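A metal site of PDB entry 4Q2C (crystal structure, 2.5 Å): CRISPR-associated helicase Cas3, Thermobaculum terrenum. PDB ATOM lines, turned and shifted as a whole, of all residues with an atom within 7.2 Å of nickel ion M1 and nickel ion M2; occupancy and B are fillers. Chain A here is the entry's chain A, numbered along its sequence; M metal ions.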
ATOM      1  N   ALA A  41     -25.667 -18.059  -6.414  1.00  0.00           N
ATOM      2  CA  ALA A  41     -26.356 -19.318  -6.100  1.00  0.00           C
ATOM      3  C   ALA A  41     -26.043 -19.786  -4.675  1.00  0.00           C
ATOM      4  O   ALA A  41     -26.872 -20.425  -4.033  1.00  0.00           O
ATOM      5  CB  ALA A  41     -25.982 -20.392  -7.100  1.00  0.00           C
ATOM      6  N   LYS A  42     -24.850 -19.465  -4.200  1.00  0.00           N
ATOM      7  CA  LYS A  42     -24.446 -19.791  -2.836  1.00  0.00           C
ATOM      8  C   LYS A  42     -23.887 -18.549  -2.171  1.00  0.00           C
ATOM      9  O   LYS A  42     -23.279 -17.696  -2.822  1.00  0.00           O
ATOM     10  CB  LYS A  42     -23.377 -20.886  -2.825  1.00  0.00           C
ATOM     11  CG  LYS A  42     -23.684 -22.106  -3.665  1.00  0.00           C
ATOM     12  CD  LYS A  42     -24.584 -23.099  -2.941  1.00  0.00           C
ATOM     13  CE  LYS A  42     -24.566 -24.450  -3.645  1.00  0.00           C
ATOM     14  NZ  LYS A  42     -25.339 -25.493  -2.920  1.00  0.00           N
ATOM     15  N   LEU A  54     -24.011 -17.940  -9.705  1.00  0.00           N
ATOM     16  CA  LEU A  54     -24.947 -18.952 -10.192  1.00  0.00           C
ATOM     17  C   LEU A  54     -24.472 -19.678 -11.458  1.00  0.00           C
ATOM     18  O   LEU A  54     -24.669 -20.884 -11.601  1.00  0.00           O
ATOM     19  CB  LEU A  54     -26.318 -18.341 -10.442  1.00  0.00           C
ATOM     20  CG  LEU A  54     -27.365 -19.177 -11.180  1.00  0.00           C
ATOM     21  CD1 LEU A  54     -27.746 -20.421 -10.391  1.00  0.00           C
ATOM     22  CD2 LEU A  54     -28.600 -18.354 -11.525  1.00  0.00           C
ATOM     23  N   HIS A  57     -22.135 -22.285 -10.387  1.00  0.00           N
ATOM     24  CA  HIS A  57     -22.793 -23.432  -9.786  1.00  0.00           C
ATOM     25  C   HIS A  57     -23.403 -24.336 -10.854  1.00  0.00           C
ATOM     26  O   HIS A  57     -23.324 -25.566 -10.760  1.00  0.00           O
ATOM     27  CB  HIS A  57     -23.876 -22.966  -8.804  1.00  0.00           C
ATOM     28  CG  HIS A  57     -24.635 -24.096  -8.176  1.00  0.00           C
ATOM     29  ND1 HIS A  57     -24.023 -25.090  -7.447  1.00  0.00           N
ATOM     30  CD2 HIS A  57     -25.964 -24.382  -8.170  1.00  0.00           C
ATOM     31  CE1 HIS A  57     -24.935 -25.946  -7.021  1.00  0.00           C
ATOM     32  NE2 HIS A  57     -26.122 -25.540  -7.436  1.00  0.00           N
ATOM     33  N   MET A  58     -23.997 -23.723 -11.877  1.00  0.00           N
ATOM     34  CA  MET A  58     -24.585 -24.494 -12.954  1.00  0.00           C
ATOM     35  C   MET A  58     -23.506 -25.235 -13.732  1.00  0.00           C
ATOM     36  O   MET A  58     -23.688 -26.402 -14.117  1.00  0.00           O
ATOM     37  CB  MET A  58     -25.391 -23.577 -13.884  1.00  0.00           C
ATOM     38  CG  MET A  58     -26.530 -22.861 -13.189  1.00  0.00           C
ATOM     39  SD  MET A  58     -27.787 -22.001 -14.416  1.00  0.00           S
ATOM     40  CE  MET A  58     -26.608 -20.607 -15.108  1.00  0.00           C
ATOM     41  N   VAL A  61     -22.444 -28.283 -11.433  1.00  0.00           N
ATOM     42  CA  VAL A  61     -23.353 -29.419 -11.493  1.00  0.00           C
ATOM     43  C   VAL A  61     -23.296 -30.102 -12.858  1.00  0.00           C
ATOM     44  O   VAL A  61     -23.355 -31.339 -12.950  1.00  0.00           O
ATOM     45  CB  VAL A  61     -24.800 -29.001 -11.135  1.00  0.00           C
ATOM     46  CG1 VAL A  61     -25.743 -30.172 -11.241  1.00  0.00           C
ATOM     47  CG2 VAL A  61     -24.840 -28.409  -9.731  1.00  0.00           C
ATOM     48  N   ALA A 100     -29.151 -30.752 -15.823  1.00  0.00           N
ATOM     49  CA  ALA A 100     -28.654 -30.824 -14.446  1.00  0.00           C
ATOM     50  C   ALA A 100     -28.077 -29.491 -14.018  1.00  0.00           C
ATOM     51  O   ALA A 100     -28.292 -29.047 -12.898  1.00  0.00           O
ATOM     52  CB  ALA A 100     -27.617 -31.930 -14.325  1.00  0.00           C
ATOM     53  N   GLY A 101     -27.368 -28.838 -14.930  1.00  0.00           N
ATOM     54  CA  GLY A 101     -26.804 -27.537 -14.619  1.00  0.00           C
ATOM     55  C   GLY A 101     -27.927 -26.528 -14.501  1.00  0.00           C
ATOM     56  O   GLY A 101     -27.865 -25.595 -13.699  1.00  0.00           O
ATOM     57  N   HIS A 103     -30.765 -26.859 -13.301  1.00  0.00           N
ATOM     58  CA  HIS A 103     -31.630 -27.060 -12.137  1.00  0.00           C
ATOM     59  C   HIS A 103     -31.870 -25.806 -11.285  1.00  0.00           C
ATOM     60  O   HIS A 103     -32.923 -25.666 -10.667  1.00  0.00           O
ATOM     61  CB  HIS A 103     -31.032 -28.129 -11.228  1.00  0.00           C
ATOM     62  CG  HIS A 103     -29.941 -27.620 -10.339  1.00  0.00           C
ATOM     63  ND1 HIS A 103     -28.684 -27.321 -10.808  1.00  0.00           N
ATOM     64  CD2 HIS A 103     -29.929 -27.340  -9.011  1.00  0.00           C
ATOM     65  CE1 HIS A 103     -27.929 -26.888  -9.800  1.00  0.00           C
ATOM     66  NE2 HIS A 103     -28.667 -26.896  -8.709  1.00  0.00           N
ATOM     67  N   ASP A 104     -30.890 -24.901 -11.240  1.00  0.00           N
ATOM     68  CA  ASP A 104     -30.979 -23.729 -10.373  1.00  0.00           C
ATOM     69  C   ASP A 104     -31.232 -22.418 -11.119  1.00  0.00           C
ATOM     70  O   ASP A 104     -30.949 -21.331 -10.598  1.00  0.00           O
ATOM     71  CB  ASP A 104     -29.722 -23.584  -9.512  1.00  0.00           C
ATOM     72  CG  ASP A 104     -29.920 -24.141  -8.110  1.00  0.00           C
ATOM     73  OD1 ASP A 104     -28.912 -24.270  -7.395  1.00  0.00           O
ATOM     74  OD2 ASP A 104     -31.075 -24.441  -7.739  1.00  0.00           O
ATOM     75  N   LYS A 107     -33.038 -19.534  -9.513  1.00  0.00           N
ATOM     76  CA  LYS A 107     -32.340 -18.643  -8.598  1.00  0.00           C
ATOM     77  C   LYS A 107     -32.133 -17.260  -9.202  1.00  0.00           C
ATOM     78  O   LYS A 107     -31.962 -16.277  -8.480  1.00  0.00           O
ATOM     79  CB  LYS A 107     -31.015 -19.254  -8.140  1.00  0.00           C
ATOM     80  CG  LYS A 107     -31.179 -20.400  -7.147  1.00  0.00           C
ATOM     81  CD  LYS A 107     -29.827 -20.888  -6.641  1.00  0.00           C
ATOM     82  CE  LYS A 107     -29.994 -21.947  -5.560  1.00  0.00           C
ATOM     83  NZ  LYS A 107     -28.688 -22.416  -5.041  1.00  0.00           N
ATOM     84  N   PHE A 112     -35.271 -14.854  -5.262  1.00  0.00           N
ATOM     85  CA  PHE A 112     -34.121 -15.530  -4.679  1.00  0.00           C
ATOM     86  C   PHE A 112     -32.935 -14.606  -4.442  1.00  0.00           C
ATOM     87  O   PHE A 112     -32.267 -14.691  -3.407  1.00  0.00           O
ATOM     88  CB  PHE A 112     -33.689 -16.727  -5.536  1.00  0.00           C
ATOM     89  CG  PHE A 112     -32.638 -17.581  -4.872  1.00  0.00           C
ATOM     90  CD1 PHE A 112     -33.016 -18.603  -4.021  1.00  0.00           C
ATOM     91  CD2 PHE A 112     -31.301 -17.356  -5.104  1.00  0.00           C
ATOM     92  CE1 PHE A 112     -32.063 -19.394  -3.408  1.00  0.00           C
ATOM     93  CE2 PHE A 112     -30.341 -18.136  -4.484  1.00  0.00           C
ATOM     94  CZ  PHE A 112     -30.719 -19.159  -3.633  1.00  0.00           C
ATOM     95  N   HIS A 143     -37.148 -21.629  -5.403  1.00  0.00           N
ATOM     96  CA  HIS A 143     -36.448 -21.443  -6.667  1.00  0.00           C
ATOM     97  C   HIS A 143     -36.600 -22.607  -7.643  1.00  0.00           C
ATOM     98  O   HIS A 143     -36.470 -22.413  -8.848  1.00  0.00           O
ATOM     99  CB  HIS A 143     -34.968 -21.098  -6.434  1.00  0.00           C
ATOM    100  CG  HIS A 143     -34.173 -22.203  -5.809  1.00  0.00           C
ATOM    101  ND1 HIS A 143     -34.050 -22.351  -4.443  1.00  0.00           N
ATOM    102  CD2 HIS A 143     -33.454 -23.198  -6.369  1.00  0.00           C
ATOM    103  CE1 HIS A 143     -33.280 -23.394  -4.193  1.00  0.00           C
ATOM    104  NE2 HIS A 143     -32.903 -23.930  -5.338  1.00  0.00           N
ATOM    105  N   GLY A 144     -36.874 -23.800  -7.131  1.00  0.00           N
ATOM    106  CA  GLY A 144     -37.043 -24.959  -7.993  1.00  0.00           C
ATOM    107  C   GLY A 144     -38.337 -24.896  -8.791  1.00  0.00           C
ATOM    108  O   GLY A 144     -38.388 -25.277  -9.965  1.00  0.00           O
ATOM    109  N   SER A 147     -37.770 -22.578 -11.409  1.00  0.00           N
ATOM    110  CA  SER A 147     -36.949 -23.213 -12.436  1.00  0.00           C
ATOM    111  C   SER A 147     -37.832 -24.007 -13.371  1.00  0.00           C
ATOM    112  O   SER A 147     -37.632 -23.985 -14.593  1.00  0.00           O
ATOM    113  CB  SER A 147     -35.901 -24.128 -11.805  1.00  0.00           C
ATOM    114  OG  SER A 147     -34.823 -23.397 -11.259  1.00  0.00           O
ATOM    115  N   VAL A 173     -36.360 -31.612 -13.118  1.00  0.00           N
ATOM    116  CA  VAL A 173     -35.236 -30.796 -12.678  1.00  0.00           C
ATOM    117  C   VAL A 173     -35.637 -29.851 -11.551  1.00  0.00           C
ATOM    118  O   VAL A 173     -34.847 -29.547 -10.658  1.00  0.00           O
ATOM    119  CB  VAL A 173     -34.632 -30.028 -13.883  1.00  0.00           C
ATOM    120  CG1 VAL A 173     -34.407 -28.564 -13.549  1.00  0.00           C
ATOM    121  CG2 VAL A 173     -33.370 -30.708 -14.379  1.00  0.00           C
ATOM    122  N   HIS A 176     -35.578 -30.892  -7.485  1.00  0.00           N
ATOM    123  CA  HIS A 176     -34.298 -31.344  -6.922  1.00  0.00           C
ATOM    124  C   HIS A 176     -34.167 -31.231  -5.396  1.00  0.00           C
ATOM    125  O   HIS A 176     -33.389 -31.956  -4.793  1.00  0.00           O
ATOM    126  CB  HIS A 176     -33.118 -30.647  -7.608  1.00  0.00           C
ATOM    127  CG  HIS A 176     -33.084 -29.167  -7.402  1.00  0.00           C
ATOM    128  ND1 HIS A 176     -33.661 -28.275  -8.288  1.00  0.00           N
ATOM    129  CD2 HIS A 176     -32.534 -28.403  -6.426  1.00  0.00           C
ATOM    130  CE1 HIS A 176     -33.469 -27.036  -7.863  1.00  0.00           C
ATOM    131  NE2 HIS A 176     -32.788 -27.093  -6.733  1.00  0.00           N
ATOM    132  N   HIS A 177     -34.916 -30.324  -4.786  1.00  0.00           N
ATOM    133  CA  HIS A 177     -34.835 -30.138  -3.344  1.00  0.00           C
ATOM    134  C   HIS A 177     -35.673 -31.097  -2.493  1.00  0.00           C
ATOM    135  O   HIS A 177     -35.651 -31.014  -1.265  1.00  0.00           O
ATOM    136  CB  HIS A 177     -35.094 -28.689  -2.952  1.00  0.00           C
ATOM    137  CG  HIS A 177     -33.919 -27.795  -3.124  1.00  0.00           C
ATOM    138  ND1 HIS A 177     -32.708 -28.048  -2.512  1.00  0.00           N
ATOM    139  CD2 HIS A 177     -33.740 -26.672  -3.867  1.00  0.00           C
ATOM    140  CE1 HIS A 177     -31.833 -27.108  -2.855  1.00  0.00           C
ATOM    141  NE2 HIS A 177     -32.435 -26.271  -3.674  1.00  0.00           N
ATOM    142  N   VAL A 238     -30.200 -35.407 -10.908  1.00  0.00           N
ATOM    143  CA  VAL A 238     -29.994 -33.965 -10.747  1.00  0.00           C
ATOM    144  C   VAL A 238     -29.749 -33.613  -9.279  1.00  0.00           C
ATOM    145  O   VAL A 238     -28.828 -32.838  -8.969  1.00  0.00           O
ATOM    146  CB  VAL A 238     -31.180 -33.155 -11.317  1.00  0.00           C
ATOM    147  CG1 VAL A 238     -30.997 -31.678 -11.037  1.00  0.00           C
ATOM    148  CG2 VAL A 238     -31.321 -33.409 -12.801  1.00  0.00           C
ATOM    149  N   ALA A 241     -26.229 -34.706  -8.285  1.00  0.00           N
ATOM    150  CA  ALA A 241     -25.208 -33.837  -8.852  1.00  0.00           C
ATOM    151  C   ALA A 241     -25.145 -32.506  -8.103  1.00  0.00           C
ATOM    152  O   ALA A 241     -24.068 -31.950  -7.893  1.00  0.00           O
ATOM    153  CB  ALA A 241     -25.456 -33.620 -10.329  1.00  0.00           C
ATOM    154  N   ASP A 242     -26.301 -32.028  -7.658  1.00  0.00           N
ATOM    155  CA  ASP A 242     -26.315 -30.818  -6.835  1.00  0.00           C
ATOM    156  C   ASP A 242     -25.641 -31.024  -5.475  1.00  0.00           C
ATOM    157  O   ASP A 242     -24.933 -30.141  -4.980  1.00  0.00           O
ATOM    158  CB  ASP A 242     -27.734 -30.290  -6.664  1.00  0.00           C
ATOM    159  CG  ASP A 242     -27.779 -28.988  -5.884  1.00  0.00           C
ATOM    160  OD1 ASP A 242     -28.309 -28.973  -4.762  1.00  0.00           O
ATOM    161  OD2 ASP A 242     -27.274 -27.974  -6.409  1.00  0.00           O
ATOM    162  N   TRP A 243     -25.834 -32.205  -4.880  1.00  0.00           N
ATOM    163  CA  TRP A 243     -25.172 -32.514  -3.614  1.00  0.00           C
ATOM    164  C   TRP A 243     -23.659 -32.532  -3.793  1.00  0.00           C
ATOM    165  O   TRP A 243     -22.915 -31.987  -2.970  1.00  0.00           O
ATOM    166  CB  TRP A 243     -25.625 -33.860  -3.043  1.00  0.00           C
ATOM    167  CG  TRP A 243     -27.080 -33.916  -2.680  1.00  0.00           C
ATOM    168  CD1 TRP A 243     -27.925 -32.869  -2.488  1.00  0.00           C
ATOM    169  CD2 TRP A 243     -27.860 -35.108  -2.492  1.00  0.00           C
ATOM    170  NE1 TRP A 243     -29.186 -33.325  -2.185  1.00  0.00           N
ATOM    171  CE2 TRP A 243     -29.167 -34.696  -2.183  1.00  0.00           C
ATOM    172  CE3 TRP A 243     -27.569 -36.471  -2.555  1.00  0.00           C
ATOM    173  CZ2 TRP A 243     -30.205 -35.612  -1.929  1.00  0.00           C
ATOM    174  CZ3 TRP A 243     -28.589 -37.382  -2.313  1.00  0.00           C
ATOM    175  CH2 TRP A 243     -29.888 -36.942  -1.996  1.00  0.00           C
ATOM    176  N   GLY A 245     -22.080 -30.891  -5.992  1.00  0.00           N
ATOM    177  CA  GLY A 245     -21.680 -29.527  -6.271  1.00  0.00           C
ATOM    178  C   GLY A 245     -21.738 -28.637  -5.042  1.00  0.00           C
ATOM    179  O   GLY A 245     -21.249 -27.505  -5.063  1.00  0.00           O
ATOM    180  N   SER A 246     -22.346 -29.135  -3.966  1.00  0.00           N
ATOM    181  CA  SER A 246     -22.476 -28.344  -2.749  1.00  0.00           C
ATOM    182  C   SER A 246     -21.370 -28.571  -1.716  1.00  0.00           C
ATOM    183  O   SER A 246     -21.403 -27.988  -0.621  1.00  0.00           O
ATOM    184  CB  SER A 246     -23.853 -28.558  -2.120  1.00  0.00           C
ATOM    185  OG  SER A 246     -24.874 -28.053  -2.975  1.00  0.00           O
ATOM    186  N   GLY A 418     -24.846 -24.770   1.951  1.00  0.00           N
ATOM    187  CA  GLY A 418     -25.556 -23.956   0.989  1.00  0.00           C
ATOM    188  C   GLY A 418     -26.570 -24.718   0.162  1.00  0.00           C
ATOM    189  O   GLY A 418     -26.713 -24.470  -1.031  1.00  0.00           O
ATOM    190  N   VAL A 419     -27.244 -25.685   0.775  1.00  0.00           N
ATOM    191  CA  VAL A 419     -28.364 -26.347   0.114  1.00  0.00           C
ATOM    192  C   VAL A 419     -29.645 -25.617   0.488  1.00  0.00           C
ATOM    193  O   VAL A 419     -30.145 -25.743   1.613  1.00  0.00           O
ATOM    194  CB  VAL A 419     -28.464 -27.833   0.492  1.00  0.00           C
ATOM    195  CG1 VAL A 419     -29.717 -28.455  -0.104  1.00  0.00           C
ATOM    196  CG2 VAL A 419     -27.207 -28.573   0.022  1.00  0.00           C
ATOM    197  N   TYR A 420     -30.174 -24.835  -0.449  1.00  0.00           N
ATOM    198  CA  TYR A 420     -31.263 -23.904  -0.163  1.00  0.00           C
ATOM    199  C   TYR A 420     -32.638 -24.557  -0.243  1.00  0.00           C
ATOM    200  O   TYR A 420     -33.459 -24.178  -1.092  1.00  0.00           O
ATOM    201  CB  TYR A 420     -31.180 -22.681  -1.078  1.00  0.00           C
ATOM    202  CG  TYR A 420     -30.052 -21.745  -0.717  1.00  0.00           C
ATOM    203  CD1 TYR A 420     -28.731 -22.115  -0.879  1.00  0.00           C
ATOM    204  CD2 TYR A 420     -30.314 -20.479  -0.194  1.00  0.00           C
ATOM    205  CE1 TYR A 420     -27.694 -21.269  -0.540  1.00  0.00           C
ATOM    206  CE2 TYR A 420     -29.287 -19.619   0.135  1.00  0.00           C
ATOM    207  CZ  TYR A 420     -27.977 -20.030  -0.029  1.00  0.00           C
ATOM    208  OH  TYR A 420     -26.955 -19.177   0.315  1.00  0.00           O
ATOM    209  N   ASP A 421     -32.891 -25.526   0.626  1.00  0.00           N
ATOM    210  CA  ASP A 421     -34.200 -26.170   0.676  1.00  0.00           C
ATOM    211  C   ASP A 421     -35.248 -25.160   1.127  1.00  0.00           C
ATOM    212  O   ASP A 421     -35.067 -24.470   2.128  1.00  0.00           O
ATOM    213  CB  ASP A 421     -34.168 -27.352   1.640  1.00  0.00           C
ATOM    214  CG  ASP A 421     -35.282 -28.355   1.386  1.00  0.00           C
ATOM    215  OD1 ASP A 421     -36.404 -27.931   1.060  1.00  0.00           O
ATOM    216  OD2 ASP A 421     -35.025 -29.572   1.511  1.00  0.00           O
HETATM  217 NI    NI M   1     -31.670 -25.568  -5.713  1.00  0.00          NI
HETATM  218 NI    NI M   2     -27.957 -26.065  -6.780  1.00  0.00          NI
HETATM  219 NI    NI M   3     -28.973 -25.688  -4.216  1.00  0.00          NI
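The side-chain hydroxyl (OG) of Ser 246 sits at hydrogen-bond distance from the backbone carbonyl oxygen (O) of Asp 242 (2.9 Å). The side-chain hydroxyl of Ser 147 lies within hydrogen-bond range of the backbone carbonyl oxygen of His 143 (3.1 Å). The side-chain amino group (NZ) of Lys 107 sits close to the side-chain carboxylate (OD1) of Asp 104. ND1 of His 176 sits at hydrogen-bond distance from O of Val 173. The backbone carbonyl oxygen of His 103 lies within hydrogen-bond range of the side-chain hydroxyl of Ser 147 (3.0 Å). ND1 of His 103 lies within hydrogen-bond range of O of Ala 100 (2.7 Å). ND1 of His 103 is in hydrogen-bond range of O of Gly 101, 3.5 Å away. The backbone carbonyl oxygen (O) of Tyr 420 sits close to a ring nitrogen (NE2) of His 177, 3.5 Å away.
Lys 107 touches nickel ion M1. Along chain A the residues within 4 Å of nickel ion M1 span positions 104 to 177. The nearest printed residue that does not touch nickel ion M1 is His 103 (4.1 Å).
Four residues have an atom within 4 Å of nickel ion M2: His 57, His 103, Asp 104 and Asp 242. The nearest printed residue that does not touch nickel ion M2 is Lys 107 (4.1 Å).
A ring nitrogen (NE2) of His 143 is bound to nickel ion M1 (2.1 Å). Nickel ion M1 is bound by a ring nitrogen (NE2) of His 176, 2.1 Å away. A ring nitrogen (NE2) of His 177 binds nickel ion M1 (2.3 Å). Nickel ion M1 is bound by OD2 of Asp 104 (2.4 Å).
Nickel ion M2 is bound by NE2 of His 57, OD2 of Asp 242, OD1 of Asp 104 and NE2 of His 103. Nickel ion M2 has four donor atoms within binding distance.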
